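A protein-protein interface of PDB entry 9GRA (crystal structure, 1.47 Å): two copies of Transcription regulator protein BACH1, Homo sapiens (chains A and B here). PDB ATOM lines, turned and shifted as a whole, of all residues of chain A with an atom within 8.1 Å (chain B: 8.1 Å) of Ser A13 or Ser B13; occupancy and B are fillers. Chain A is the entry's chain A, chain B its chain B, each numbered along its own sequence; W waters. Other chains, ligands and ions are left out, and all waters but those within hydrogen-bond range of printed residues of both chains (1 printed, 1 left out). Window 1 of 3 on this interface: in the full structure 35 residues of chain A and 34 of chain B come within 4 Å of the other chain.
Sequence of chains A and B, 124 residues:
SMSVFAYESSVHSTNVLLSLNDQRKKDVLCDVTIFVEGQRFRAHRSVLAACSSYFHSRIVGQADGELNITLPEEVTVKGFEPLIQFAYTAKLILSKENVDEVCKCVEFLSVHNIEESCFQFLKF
Ser A13 touches just these residues of chain B: Ser B13, Thr B14 and Leu B17. Of the printed residues of chain A, Ser B13 touches Ser A13 (2.9 Å), Thr A14 (3.3 Å) and Leu A17 (3.8 Å). Printed residues of chain A within 4 Å of Ser B9: Phe A86 (3.9 Å) and Ala A90 (2.9 Å). Of the printed residues of chain B, Leu A17 touches His B12 and Ser B13. Of the printed residues of chain B, His A12 touches Leu B17, Phe B86, Ala B87 and Ala B90. Ser B19 touches none of the printed residues of chain A. Leu A18 touches none of the printed residues of chain B.
Of the 17 printed residues of chain B, 8 touch a printed residue of chain A. Hydrophobic or aromatic side chains of chain A within 4 Å of the printed part of chain B: His A12, Leu A17, Phe A86 and Ala A90.
Ser A9 touches Ala B90, and with the chains exchanged Ala A90 touches Ser B9. Ser B13 touches its own counterpart, Ser A13. Ser A13 touches Thr B14, and with the chains exchanged Thr A14 touches Ser B13. Ser A13 touches Leu B17, and with the chains exchanged Leu A17 touches Ser B13. Positions printed for both chains: 9, 10, 11, 12, 13, 14, 15, 16, 17, 18, 19, 20, 86, 87, 88, 89 and 90. Of the 16 pairs that touch across the chains among the printed residues, 15 have their exchanged pair printed and touching as well.
Leu B17 touches His A12 (CD2 to CD2, 3.8 Å). His A12 touches Phe B86 (NE2 to O, 3.5 Å). Ala B90 touches His A12. CD2 of Leu B17 touches CB of Ser A13, 3.9 Å away. Leu A17 touches His B12. Leu A17 touches Ser B13 (CD2 to CB, 3.8 Å). Ser B9 touches Phe A86. CB of Ala A90 touches CB of His B12, at 3.7 Å.
The side-chain hydroxyl (OG) of Ser A9 sits close to the backbone NH (N) of Val A11 (3.4 Å). OG of Ser A9 sits at hydrogen-bond distance from N of His A12 (3.0 Å). The side-chain hydroxyl (OG) of Ser B9 is in hydrogen-bond range of the backbone NH (N) of Val B11, 3.2 Å away. The backbone NH (N) of His B12 lies within hydrogen-bond range of the side-chain hydroxyl (OG) of Ser B9, at 3.1 Å.
N of Ser A9 lies within hydrogen-bond range of O of Ala B90, at 2.9 Å. O of Ala B87 is in hydrogen-bond range of NE2 of His A12 (2.8 Å). OG of Ser A13 sits at hydrogen-bond distance from OG of Ser B13 (2.9 Å). The side-chain hydroxyl (OG) of Ser A13 is in hydrogen-bond range of the side-chain hydroxyl (OG1) of Thr B14, at 3.3 Å. The side-chain hydroxyl of Thr A14 lies within hydrogen-bond range of the side-chain hydroxyl of Ser B13. The backbone carbonyl oxygen (O) of Phe A86 is in hydrogen-bond range of a ring nitrogen (NE2) of His B12 (3.5 Å). O of Ala A87 lies within hydrogen-bond range of NE2 of His B12 (2.7 Å). The backbone carbonyl oxygen (O) of Ala A90 is in hydrogen-bond range of the backbone NH (N) of Ser B9 (2.9 Å).
Water W1 bridges OG1 of Thr A14 and OG of Ser B13.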
ATOM      1  N   SER A   9      -6.725 -14.230  16.649  1.00  0.00           N
ATOM      2  CA  SER A   9      -6.399 -13.519  15.418  1.00  0.00           C
ATOM      3  C   SER A   9      -6.491 -14.505  14.255  1.00  0.00           C
ATOM      4  O   SER A   9      -5.788 -15.529  14.251  1.00  0.00           O
ATOM      5  CB  SER A   9      -4.971 -12.984  15.488  1.00  0.00           C
ATOM      6  OG  SER A   9      -4.614 -12.447  14.208  1.00  0.00           O
ATOM      7  N   SER A  10      -7.344 -14.208  13.272  1.00  0.00           N
ATOM      8  CA  SER A  10      -7.429 -15.122  12.140  1.00  0.00           C
ATOM      9  C   SER A  10      -6.273 -14.950  11.152  1.00  0.00           C
ATOM     10  O   SER A  10      -6.096 -15.817  10.281  1.00  0.00           O
ATOM     11  CB  SER A  10      -8.741 -14.964  11.372  1.00  0.00           C
ATOM     12  OG  SER A  10      -8.736 -13.740  10.686  1.00  0.00           O
ATOM     13  N   VAL A  11      -5.513 -13.848  11.241  1.00  0.00           N
ATOM     14  CA  VAL A  11      -4.437 -13.518  10.297  1.00  0.00           C
ATOM     15  C   VAL A  11      -3.049 -13.760  10.873  1.00  0.00           C
ATOM     16  O   VAL A  11      -2.074 -13.787  10.112  1.00  0.00           O
ATOM     17  CB  VAL A  11      -4.576 -12.048   9.846  1.00  0.00           C
ATOM     18  CG1 VAL A  11      -6.003 -11.799   9.273  1.00  0.00           C
ATOM     19  CG2 VAL A  11      -4.257 -11.058  10.991  1.00  0.00           C
ATOM     20  N   HIS A  12      -2.923 -13.945  12.188  1.00  0.00           N
ATOM     21  CA  HIS A  12      -1.584 -13.966  12.767  1.00  0.00           C
ATOM     22  C   HIS A  12      -0.701 -15.058  12.162  1.00  0.00           C
ATOM     23  O   HIS A  12       0.453 -14.801  11.840  1.00  0.00           O
ATOM     24  CB  HIS A  12      -1.651 -14.108  14.285  1.00  0.00           C
ATOM     25  CG  HIS A  12      -0.308 -14.247  14.932  1.00  0.00           C
ATOM     26  ND1 HIS A  12       0.584 -13.194  15.029  1.00  0.00           N
ATOM     27  CD2 HIS A  12       0.263 -15.292  15.582  1.00  0.00           C
ATOM     28  CE1 HIS A  12       1.670 -13.611  15.658  1.00  0.00           C
ATOM     29  NE2 HIS A  12       1.506 -14.884  15.992  1.00  0.00           N
ATOM     30  N   SER A  13      -1.176 -16.313  12.096  1.00  0.00           N
ATOM     31  CA  SER A  13      -0.300 -17.365  11.541  1.00  0.00           C
ATOM     32  C   SER A  13       0.141 -17.067  10.100  1.00  0.00           C
ATOM     33  O   SER A  13       1.291 -17.351   9.722  1.00  0.00           O
ATOM     34  CB  SER A  13      -0.954 -18.748  11.658  1.00  0.00           C
ATOM     35  OG  SER A  13      -2.093 -18.822  10.808  1.00  0.00           O
ATOM     36  N   THR A  14      -0.771 -16.509   9.293  1.00  0.00           N
ATOM     37  CA  THR A  14      -0.397 -16.090   7.941  1.00  0.00           C
ATOM     38  C   THR A  14       0.658 -15.001   7.980  1.00  0.00           C
ATOM     39  O   THR A  14       1.635 -15.033   7.209  1.00  0.00           O
ATOM     40  CB  THR A  14      -1.635 -15.610   7.244  1.00  0.00           C
ATOM     41  OG1 THR A  14      -2.513 -16.736   7.068  1.00  0.00           O
ATOM     42  CG2 THR A  14      -1.274 -15.077   5.874  1.00  0.00           C
ATOM     43  N   ASN A  15       0.513 -14.065   8.922  1.00  0.00           N
ATOM     44  CA  ASN A  15       1.478 -12.980   8.984  1.00  0.00           C
ATOM     45  C   ASN A  15       2.854 -13.472   9.415  1.00  0.00           C
ATOM     46  O   ASN A  15       3.887 -13.035   8.875  1.00  0.00           O
ATOM     47  CB  ASN A  15       0.994 -11.929   9.966  1.00  0.00           C
ATOM     48  CG  ASN A  15      -0.158 -11.119   9.428  1.00  0.00           C
ATOM     49  OD1 ASN A  15      -0.421 -11.074   8.196  1.00  0.00           O
ATOM     50  ND2 ASN A  15      -0.867 -10.471  10.350  1.00  0.00           N
ATOM     51  N   VAL A  16       2.921 -14.446  10.345  1.00  0.00           N
ATOM     52  CA  VAL A  16       4.209 -14.989  10.754  1.00  0.00           C
ATOM     53  C   VAL A  16       4.836 -15.710   9.580  1.00  0.00           C
ATOM     54  O   VAL A  16       6.017 -15.528   9.287  1.00  0.00           O
ATOM     55  CB  VAL A  16       4.047 -15.931  11.959  1.00  0.00           C
ATOM     56  CG1 VAL A  16       5.392 -16.642  12.259  1.00  0.00           C
ATOM     57  CG2 VAL A  16       3.587 -15.163  13.206  1.00  0.00           C
ATOM     58  N   LEU A  17       4.035 -16.495   8.844  1.00  0.00           N
ATOM     59  CA  LEU A  17       4.615 -17.202   7.707  1.00  0.00           C
ATOM     60  C   LEU A  17       5.096 -16.234   6.638  1.00  0.00           C
ATOM     61  O   LEU A  17       6.132 -16.479   6.026  1.00  0.00           O
ATOM     62  CB  LEU A  17       3.597 -18.167   7.120  1.00  0.00           C
ATOM     63  CG  LEU A  17       4.145 -19.295   6.251  1.00  0.00           C
ATOM     64  CD1 LEU A  17       5.147 -20.210   6.923  1.00  0.00           C
ATOM     65  CD2 LEU A  17       2.961 -20.111   5.765  1.00  0.00           C
ATOM     66  N   LEU A  18       4.360 -15.123   6.410  1.00  0.00           N
ATOM     67  CA  LEU A  18       4.807 -14.091   5.466  1.00  0.00           C
ATOM     68  C   LEU A  18       6.156 -13.542   5.887  1.00  0.00           C
ATOM     69  O   LEU A  18       7.048 -13.326   5.037  1.00  0.00           O
ATOM     70  CB  LEU A  18       3.816 -12.923   5.388  1.00  0.00           C
ATOM     71  CG  LEU A  18       2.533 -12.964   4.499  1.00  0.00           C
ATOM     72  CD1 LEU A  18       1.571 -11.844   4.894  1.00  0.00           C
ATOM     73  CD2 LEU A  18       2.792 -12.933   2.976  1.00  0.00           C
ATOM     74  N   SER A  19       6.329 -13.313   7.193  1.00  0.00           N
ATOM     75  CA  SER A  19       7.615 -12.809   7.634  1.00  0.00           C
ATOM     76  C   SER A  19       8.718 -13.823   7.442  1.00  0.00           C
ATOM     77  O   SER A  19       9.823 -13.470   7.019  1.00  0.00           O
ATOM     78  CB  SER A  19       7.508 -12.373   9.080  1.00  0.00           C
ATOM     79  OG  SER A  19       6.655 -11.245   9.152  1.00  0.00           O
ATOM     80  N   LEU A  20       8.465 -15.084   7.799  1.00  0.00           N
ATOM     81  CA  LEU A  20       9.456 -16.139   7.566  1.00  0.00           C
ATOM     82  C   LEU A  20       9.825 -16.253   6.086  1.00  0.00           C
ATOM     83  O   LEU A  20      11.004 -16.486   5.723  1.00  0.00           O
ATOM     84  CB  LEU A  20       8.895 -17.461   8.045  1.00  0.00           C
ATOM     85  CG  LEU A  20       8.745 -17.531   9.587  1.00  0.00           C
ATOM     86  CD1 LEU A  20       8.032 -18.841  10.070  1.00  0.00           C
ATOM     87  CD2 LEU A  20      10.015 -17.314  10.331  1.00  0.00           C
ATOM     88  N   PHE A  86       5.554 -23.554  -1.400  1.00  0.00           N
ATOM     89  CA  PHE A  86       4.342 -23.897  -0.640  1.00  0.00           C
ATOM     90  C   PHE A  86       4.618 -23.883   0.867  1.00  0.00           C
ATOM     91  O   PHE A  86       3.799 -23.373   1.672  1.00  0.00           O
ATOM     92  CB  PHE A  86       3.845 -25.306  -1.021  1.00  0.00           C
ATOM     93  CG  PHE A  86       2.699 -25.800  -0.122  1.00  0.00           C
ATOM     94  CD1 PHE A  86       1.409 -25.339  -0.354  1.00  0.00           C
ATOM     95  CD2 PHE A  86       2.932 -26.660   0.949  1.00  0.00           C
ATOM     96  CE1 PHE A  86       0.356 -25.700   0.474  1.00  0.00           C
ATOM     97  CE2 PHE A  86       1.869 -27.059   1.783  1.00  0.00           C
ATOM     98  CZ  PHE A  86       0.575 -26.582   1.521  1.00  0.00           C
ATOM     99  N   ALA A  87       5.761 -24.456   1.280  1.00  0.00           N
ATOM    100  CA  ALA A  87       6.031 -24.501   2.720  1.00  0.00           C
ATOM    101  C   ALA A  87       5.953 -23.108   3.335  1.00  0.00           C
ATOM    102  O   ALA A  87       5.510 -22.938   4.467  1.00  0.00           O
ATOM    103  CB  ALA A  87       7.409 -25.098   2.952  1.00  0.00           C
ATOM    104  N   TYR A  88       6.439 -22.107   2.592  1.00  0.00           N
ATOM    105  CA  TYR A  88       6.593 -20.749   3.121  1.00  0.00           C
ATOM    106  C   TYR A  88       5.469 -19.829   2.768  1.00  0.00           C
ATOM    107  O   TYR A  88       5.481 -18.672   3.221  1.00  0.00           O
ATOM    108  CB  TYR A  88       7.898 -20.169   2.661  1.00  0.00           C
ATOM    109  CG  TYR A  88       9.066 -20.546   3.595  1.00  0.00           C
ATOM    110  CD1 TYR A  88       9.809 -21.720   3.398  1.00  0.00           C
ATOM    111  CD2 TYR A  88       9.393 -19.758   4.716  1.00  0.00           C
ATOM    112  CE1 TYR A  88      10.862 -22.052   4.281  1.00  0.00           C
ATOM    113  CE2 TYR A  88      10.447 -20.101   5.592  1.00  0.00           C
ATOM    114  CZ  TYR A  88      11.156 -21.239   5.366  1.00  0.00           C
ATOM    115  OH  TYR A  88      12.201 -21.562   6.174  1.00  0.00           O
ATOM    116  N   THR A  89       4.498 -20.277   1.964  1.00  0.00           N
ATOM    117  CA  THR A  89       3.435 -19.392   1.509  1.00  0.00           C
ATOM    118  C   THR A  89       2.049 -20.007   1.530  1.00  0.00           C
ATOM    119  O   THR A  89       1.071 -19.252   1.348  1.00  0.00           O
ATOM    120  CB  THR A  89       3.633 -18.892   0.057  1.00  0.00           C
ATOM    121  OG1 THR A  89       3.430 -19.989  -0.844  1.00  0.00           O
ATOM    122  CG2 THR A  89       5.034 -18.303  -0.191  1.00  0.00           C
ATOM    123  N   ALA A  90       1.908 -21.338   1.717  1.00  0.00           N
ATOM    124  CA  ALA A  90       0.628 -22.054   1.676  1.00  0.00           C
ATOM    125  C   ALA A  90       0.020 -22.149   0.282  1.00  0.00           C
ATOM    126  O   ALA A  90      -1.138 -22.600   0.159  1.00  0.00           O
ATOM    127  CB  ALA A  90      -0.399 -21.524   2.687  1.00  0.00           C
ATOM    128  N   SER B   9      -3.807 -23.534   0.565  1.00  0.00           N
ATOM    129  CA  SER B   9      -4.245 -24.294   1.724  1.00  0.00           C
ATOM    130  C   SER B   9      -4.730 -23.320   2.791  1.00  0.00           C
ATOM    131  O   SER B   9      -4.007 -22.391   3.173  1.00  0.00           O
ATOM    132  CB  SER B   9      -3.046 -25.030   2.309  1.00  0.00           C
ATOM    133  OG  SER B   9      -3.369 -25.648   3.556  1.00  0.00           O
ATOM    134  N   SER B  10      -5.916 -23.577   3.335  1.00  0.00           N
ATOM    135  CA  SER B  10      -6.369 -22.729   4.427  1.00  0.00           C
ATOM    136  C   SER B  10      -5.824 -23.182   5.779  1.00  0.00           C
ATOM    137  O   SER B  10      -5.972 -22.442   6.764  1.00  0.00           O
ATOM    138  CB  SER B  10      -7.902 -22.718   4.496  1.00  0.00           C
ATOM    139  OG  SER B  10      -8.369 -24.015   4.763  1.00  0.00           O
ATOM    140  N   VAL B  11      -5.215 -24.369   5.867  1.00  0.00           N
ATOM    141  CA  VAL B  11      -4.729 -24.863   7.165  1.00  0.00           C
ATOM    142  C   VAL B  11      -3.217 -24.715   7.357  1.00  0.00           C
ATOM    143  O   VAL B  11      -2.728 -24.793   8.502  1.00  0.00           O
ATOM    144  CB  VAL B  11      -5.169 -26.322   7.427  1.00  0.00           C
ATOM    145  CG1 VAL B  11      -6.691 -26.431   7.331  1.00  0.00           C
ATOM    146  CG2 VAL B  11      -4.496 -27.286   6.489  1.00  0.00           C
ATOM    147  N   HIS B  12      -2.465 -24.461   6.285  1.00  0.00           N
ATOM    148  CA  HIS B  12      -1.020 -24.645   6.336  1.00  0.00           C
ATOM    149  C   HIS B  12      -0.370 -23.685   7.312  1.00  0.00           C
ATOM    150  O   HIS B  12       0.418 -24.099   8.170  1.00  0.00           O
ATOM    151  CB  HIS B  12      -0.435 -24.446   4.946  1.00  0.00           C
ATOM    152  CG  HIS B  12       1.028 -24.605   4.931  1.00  0.00           C
ATOM    153  ND1 HIS B  12       1.631 -25.836   5.085  1.00  0.00           N
ATOM    154  CD2 HIS B  12       2.031 -23.703   4.834  1.00  0.00           C
ATOM    155  CE1 HIS B  12       2.950 -25.680   5.066  1.00  0.00           C
ATOM    156  NE2 HIS B  12       3.219 -24.382   4.935  1.00  0.00           N
ATOM    157  N   SER B  13      -0.695 -22.383   7.230  1.00  0.00           N
ATOM    158  CA  SER B  13       0.038 -21.473   8.132  1.00  0.00           C
ATOM    159  C   SER B  13      -0.249 -21.780   9.611  1.00  0.00           C
ATOM    160  O   SER B  13       0.657 -21.714  10.455  1.00  0.00           O
ATOM    161  CB  SER B  13      -0.254 -20.008   7.808  1.00  0.00           C
ATOM    162  OG  SER B  13      -1.605 -19.721   8.058  1.00  0.00           O
ATOM    163  N   THR B  14      -1.502 -22.136   9.929  1.00  0.00           N
ATOM    164  CA  THR B  14      -1.866 -22.572  11.275  1.00  0.00           C
ATOM    165  C   THR B  14      -1.110 -23.819  11.666  1.00  0.00           C
ATOM    166  O   THR B  14      -0.568 -23.909  12.781  1.00  0.00           O
ATOM    167  CB  THR B  14      -3.389 -22.745  11.352  1.00  0.00           C
ATOM    168  OG1 THR B  14      -4.012 -21.480  11.129  1.00  0.00           O
ATOM    169  CG2 THR B  14      -3.912 -23.313  12.742  1.00  0.00           C
ATOM    170  N   ASN B  15      -0.973 -24.772  10.721  1.00  0.00           N
ATOM    171  CA  ASN B  15      -0.271 -26.006  11.059  1.00  0.00           C
ATOM    172  C   ASN B  15       1.226 -25.771  11.298  1.00  0.00           C
ATOM    173  O   ASN B  15       1.813 -26.377  12.217  1.00  0.00           O
ATOM    174  CB  ASN B  15      -0.543 -27.057   9.989  1.00  0.00           C
ATOM    175  CG  ASN B  15      -1.981 -27.592  10.058  1.00  0.00           C
ATOM    176  OD1 ASN B  15      -2.699 -27.334  11.025  1.00  0.00           O
ATOM    177  ND2 ASN B  15      -2.395 -28.346   9.006  1.00  0.00           N
ATOM    178  N   VAL B  16       1.862 -24.896  10.527  1.00  0.00           N
ATOM    179  CA  VAL B  16       3.271 -24.571  10.785  1.00  0.00           C
ATOM    180  C   VAL B  16       3.419 -23.935  12.166  1.00  0.00           C
ATOM    181  O   VAL B  16       4.336 -24.269  12.918  1.00  0.00           O
ATOM    182  CB  VAL B  16       3.814 -23.660   9.672  1.00  0.00           C
ATOM    183  CG1 VAL B  16       5.229 -23.172   9.991  1.00  0.00           C
ATOM    184  CG2 VAL B  16       3.807 -24.405   8.345  1.00  0.00           C
ATOM    185  N   LEU B  17       2.535 -22.971  12.496  1.00  0.00           N
ATOM    186  CA  LEU B  17       2.644 -22.314  13.806  1.00  0.00           C
ATOM    187  C   LEU B  17       2.445 -23.304  14.948  1.00  0.00           C
ATOM    188  O   LEU B  17       3.158 -23.215  15.967  1.00  0.00           O
ATOM    189  CB  LEU B  17       1.675 -21.113  13.877  1.00  0.00           C
ATOM    190  CG  LEU B  17       1.991 -20.085  14.959  1.00  0.00           C
ATOM    191  CD1 LEU B  17       3.338 -19.436  14.801  1.00  0.00           C
ATOM    192  CD2 LEU B  17       0.892 -19.010  15.073  1.00  0.00           C
ATOM    193  N   LEU B  18       1.464 -24.235  14.814  1.00  0.00           N
ATOM    194  CA  LEU B  18       1.302 -25.302  15.818  1.00  0.00           C
ATOM    195  C   LEU B  18       2.578 -26.105  15.974  1.00  0.00           C
ATOM    196  O   LEU B  18       2.959 -26.479  17.097  1.00  0.00           O
ATOM    197  CB  LEU B  18       0.198 -26.287  15.406  1.00  0.00           C
ATOM    198  CG  LEU B  18      -1.281 -25.957  15.588  1.00  0.00           C
ATOM    199  CD1 LEU B  18      -2.084 -26.936  14.723  1.00  0.00           C
ATOM    200  CD2 LEU B  18      -1.701 -26.063  17.037  1.00  0.00           C
ATOM    201  N   SER B  19       3.248 -26.410  14.866  1.00  0.00           N
ATOM    202  CA  SER B  19       4.474 -27.168  14.995  1.00  0.00           C
ATOM    203  C   SER B  19       5.567 -26.341  15.663  1.00  0.00           C
ATOM    204  O   SER B  19       6.287 -26.836  16.538  1.00  0.00           O
ATOM    205  CB  SER B  19       4.921 -27.635  13.618  1.00  0.00           C
ATOM    206  OG  SER B  19       3.949 -28.511  13.048  1.00  0.00           O
ATOM    207  N   LEU B  20       5.686 -25.061  15.297  1.00  0.00           N
ATOM    208  CA  LEU B  20       6.676 -24.211  15.950  1.00  0.00           C
ATOM    209  C   LEU B  20       6.374 -24.078  17.448  1.00  0.00           C
ATOM    210  O   LEU B  20       7.302 -24.064  18.281  1.00  0.00           O
ATOM    211  CB  LEU B  20       6.679 -22.828  15.291  1.00  0.00           C
ATOM    212  CG  LEU B  20       7.195 -22.817  13.865  1.00  0.00           C
ATOM    213  CD1 LEU B  20       6.998 -21.417  13.228  1.00  0.00           C
ATOM    214  CD2 LEU B  20       8.645 -23.297  13.802  1.00  0.00           C
ATOM    215  N   PHE B  86       0.747 -15.873  22.726  1.00  0.00           N
ATOM    216  CA  PHE B  86       0.065 -15.338  21.550  1.00  0.00           C
ATOM    217  C   PHE B  86       0.944 -15.473  20.296  1.00  0.00           C
ATOM    218  O   PHE B  86       0.444 -15.844  19.207  1.00  0.00           O
ATOM    219  CB  PHE B  86      -0.292 -13.863  21.747  1.00  0.00           C
ATOM    220  CG  PHE B  86      -0.777 -13.225  20.488  1.00  0.00           C
ATOM    221  CD1 PHE B  86      -2.074 -13.410  20.055  1.00  0.00           C
ATOM    222  CD2 PHE B  86       0.073 -12.479  19.698  1.00  0.00           C
ATOM    223  CE1 PHE B  86      -2.536 -12.845  18.844  1.00  0.00           C
ATOM    224  CE2 PHE B  86      -0.366 -11.890  18.543  1.00  0.00           C
ATOM    225  CZ  PHE B  86      -1.665 -12.090  18.077  1.00  0.00           C
ATOM    226  N   ALA B  87       2.240 -15.131  20.420  1.00  0.00           N
ATOM    227  CA  ALA B  87       3.114 -15.158  19.243  1.00  0.00           C
ATOM    228  C   ALA B  87       3.068 -16.538  18.615  1.00  0.00           C
ATOM    229  O   ALA B  87       3.100 -16.667  17.395  1.00  0.00           O
ATOM    230  CB  ALA B  87       4.550 -14.806  19.638  1.00  0.00           C
ATOM    231  N   TYR B  88       2.992 -17.589  19.452  1.00  0.00           N
ATOM    232  CA  TYR B  88       3.045 -18.956  18.947  1.00  0.00           C
ATOM    233  C   TYR B  88       1.709 -19.637  18.739  1.00  0.00           C
ATOM    234  O   TYR B  88       1.705 -20.811  18.291  1.00  0.00           O
ATOM    235  CB  TYR B  88       3.946 -19.779  19.858  1.00  0.00           C
ATOM    236  CG  TYR B  88       5.420 -19.653  19.530  1.00  0.00           C
ATOM    237  CD1 TYR B  88       6.194 -18.603  20.032  1.00  0.00           C
ATOM    238  CD2 TYR B  88       6.049 -20.560  18.713  1.00  0.00           C
ATOM    239  CE1 TYR B  88       7.557 -18.487  19.733  1.00  0.00           C
ATOM    240  CE2 TYR B  88       7.433 -20.446  18.380  1.00  0.00           C
ATOM    241  CZ  TYR B  88       8.159 -19.404  18.908  1.00  0.00           C
ATOM    242  OH  TYR B  88       9.499 -19.259  18.690  1.00  0.00           O
ATOM    243  N   THR B  89       0.566 -18.991  19.068  1.00  0.00           N
ATOM    244  CA  THR B  89      -0.732 -19.648  18.970  1.00  0.00           C
ATOM    245  C   THR B  89      -1.820 -18.808  18.340  1.00  0.00           C
ATOM    246  O   THR B  89      -2.886 -19.372  18.052  1.00  0.00           O
ATOM    247  CB  THR B  89      -1.274 -20.072  20.328  1.00  0.00           C
ATOM    248  OG1 THR B  89      -1.620 -18.907  21.094  1.00  0.00           O
ATOM    249  CG2 THR B  89      -0.317 -20.986  21.074  1.00  0.00           C
ATOM    250  N   ALA B  90      -1.630 -17.483  18.162  1.00  0.00           N
ATOM    251  CA  ALA B  90      -2.632 -16.552  17.639  1.00  0.00           C
ATOM    252  C   ALA B  90      -3.757 -16.305  18.640  1.00  0.00           C
ATOM    253  O   ALA B  90      -4.780 -15.714  18.282  1.00  0.00           O
ATOM    254  CB  ALA B  90      -3.190 -16.988  16.265  1.00  0.00           C
HETATM  255  O   HOH W   1      -2.105 -18.666   5.111  1.00  0.00           O
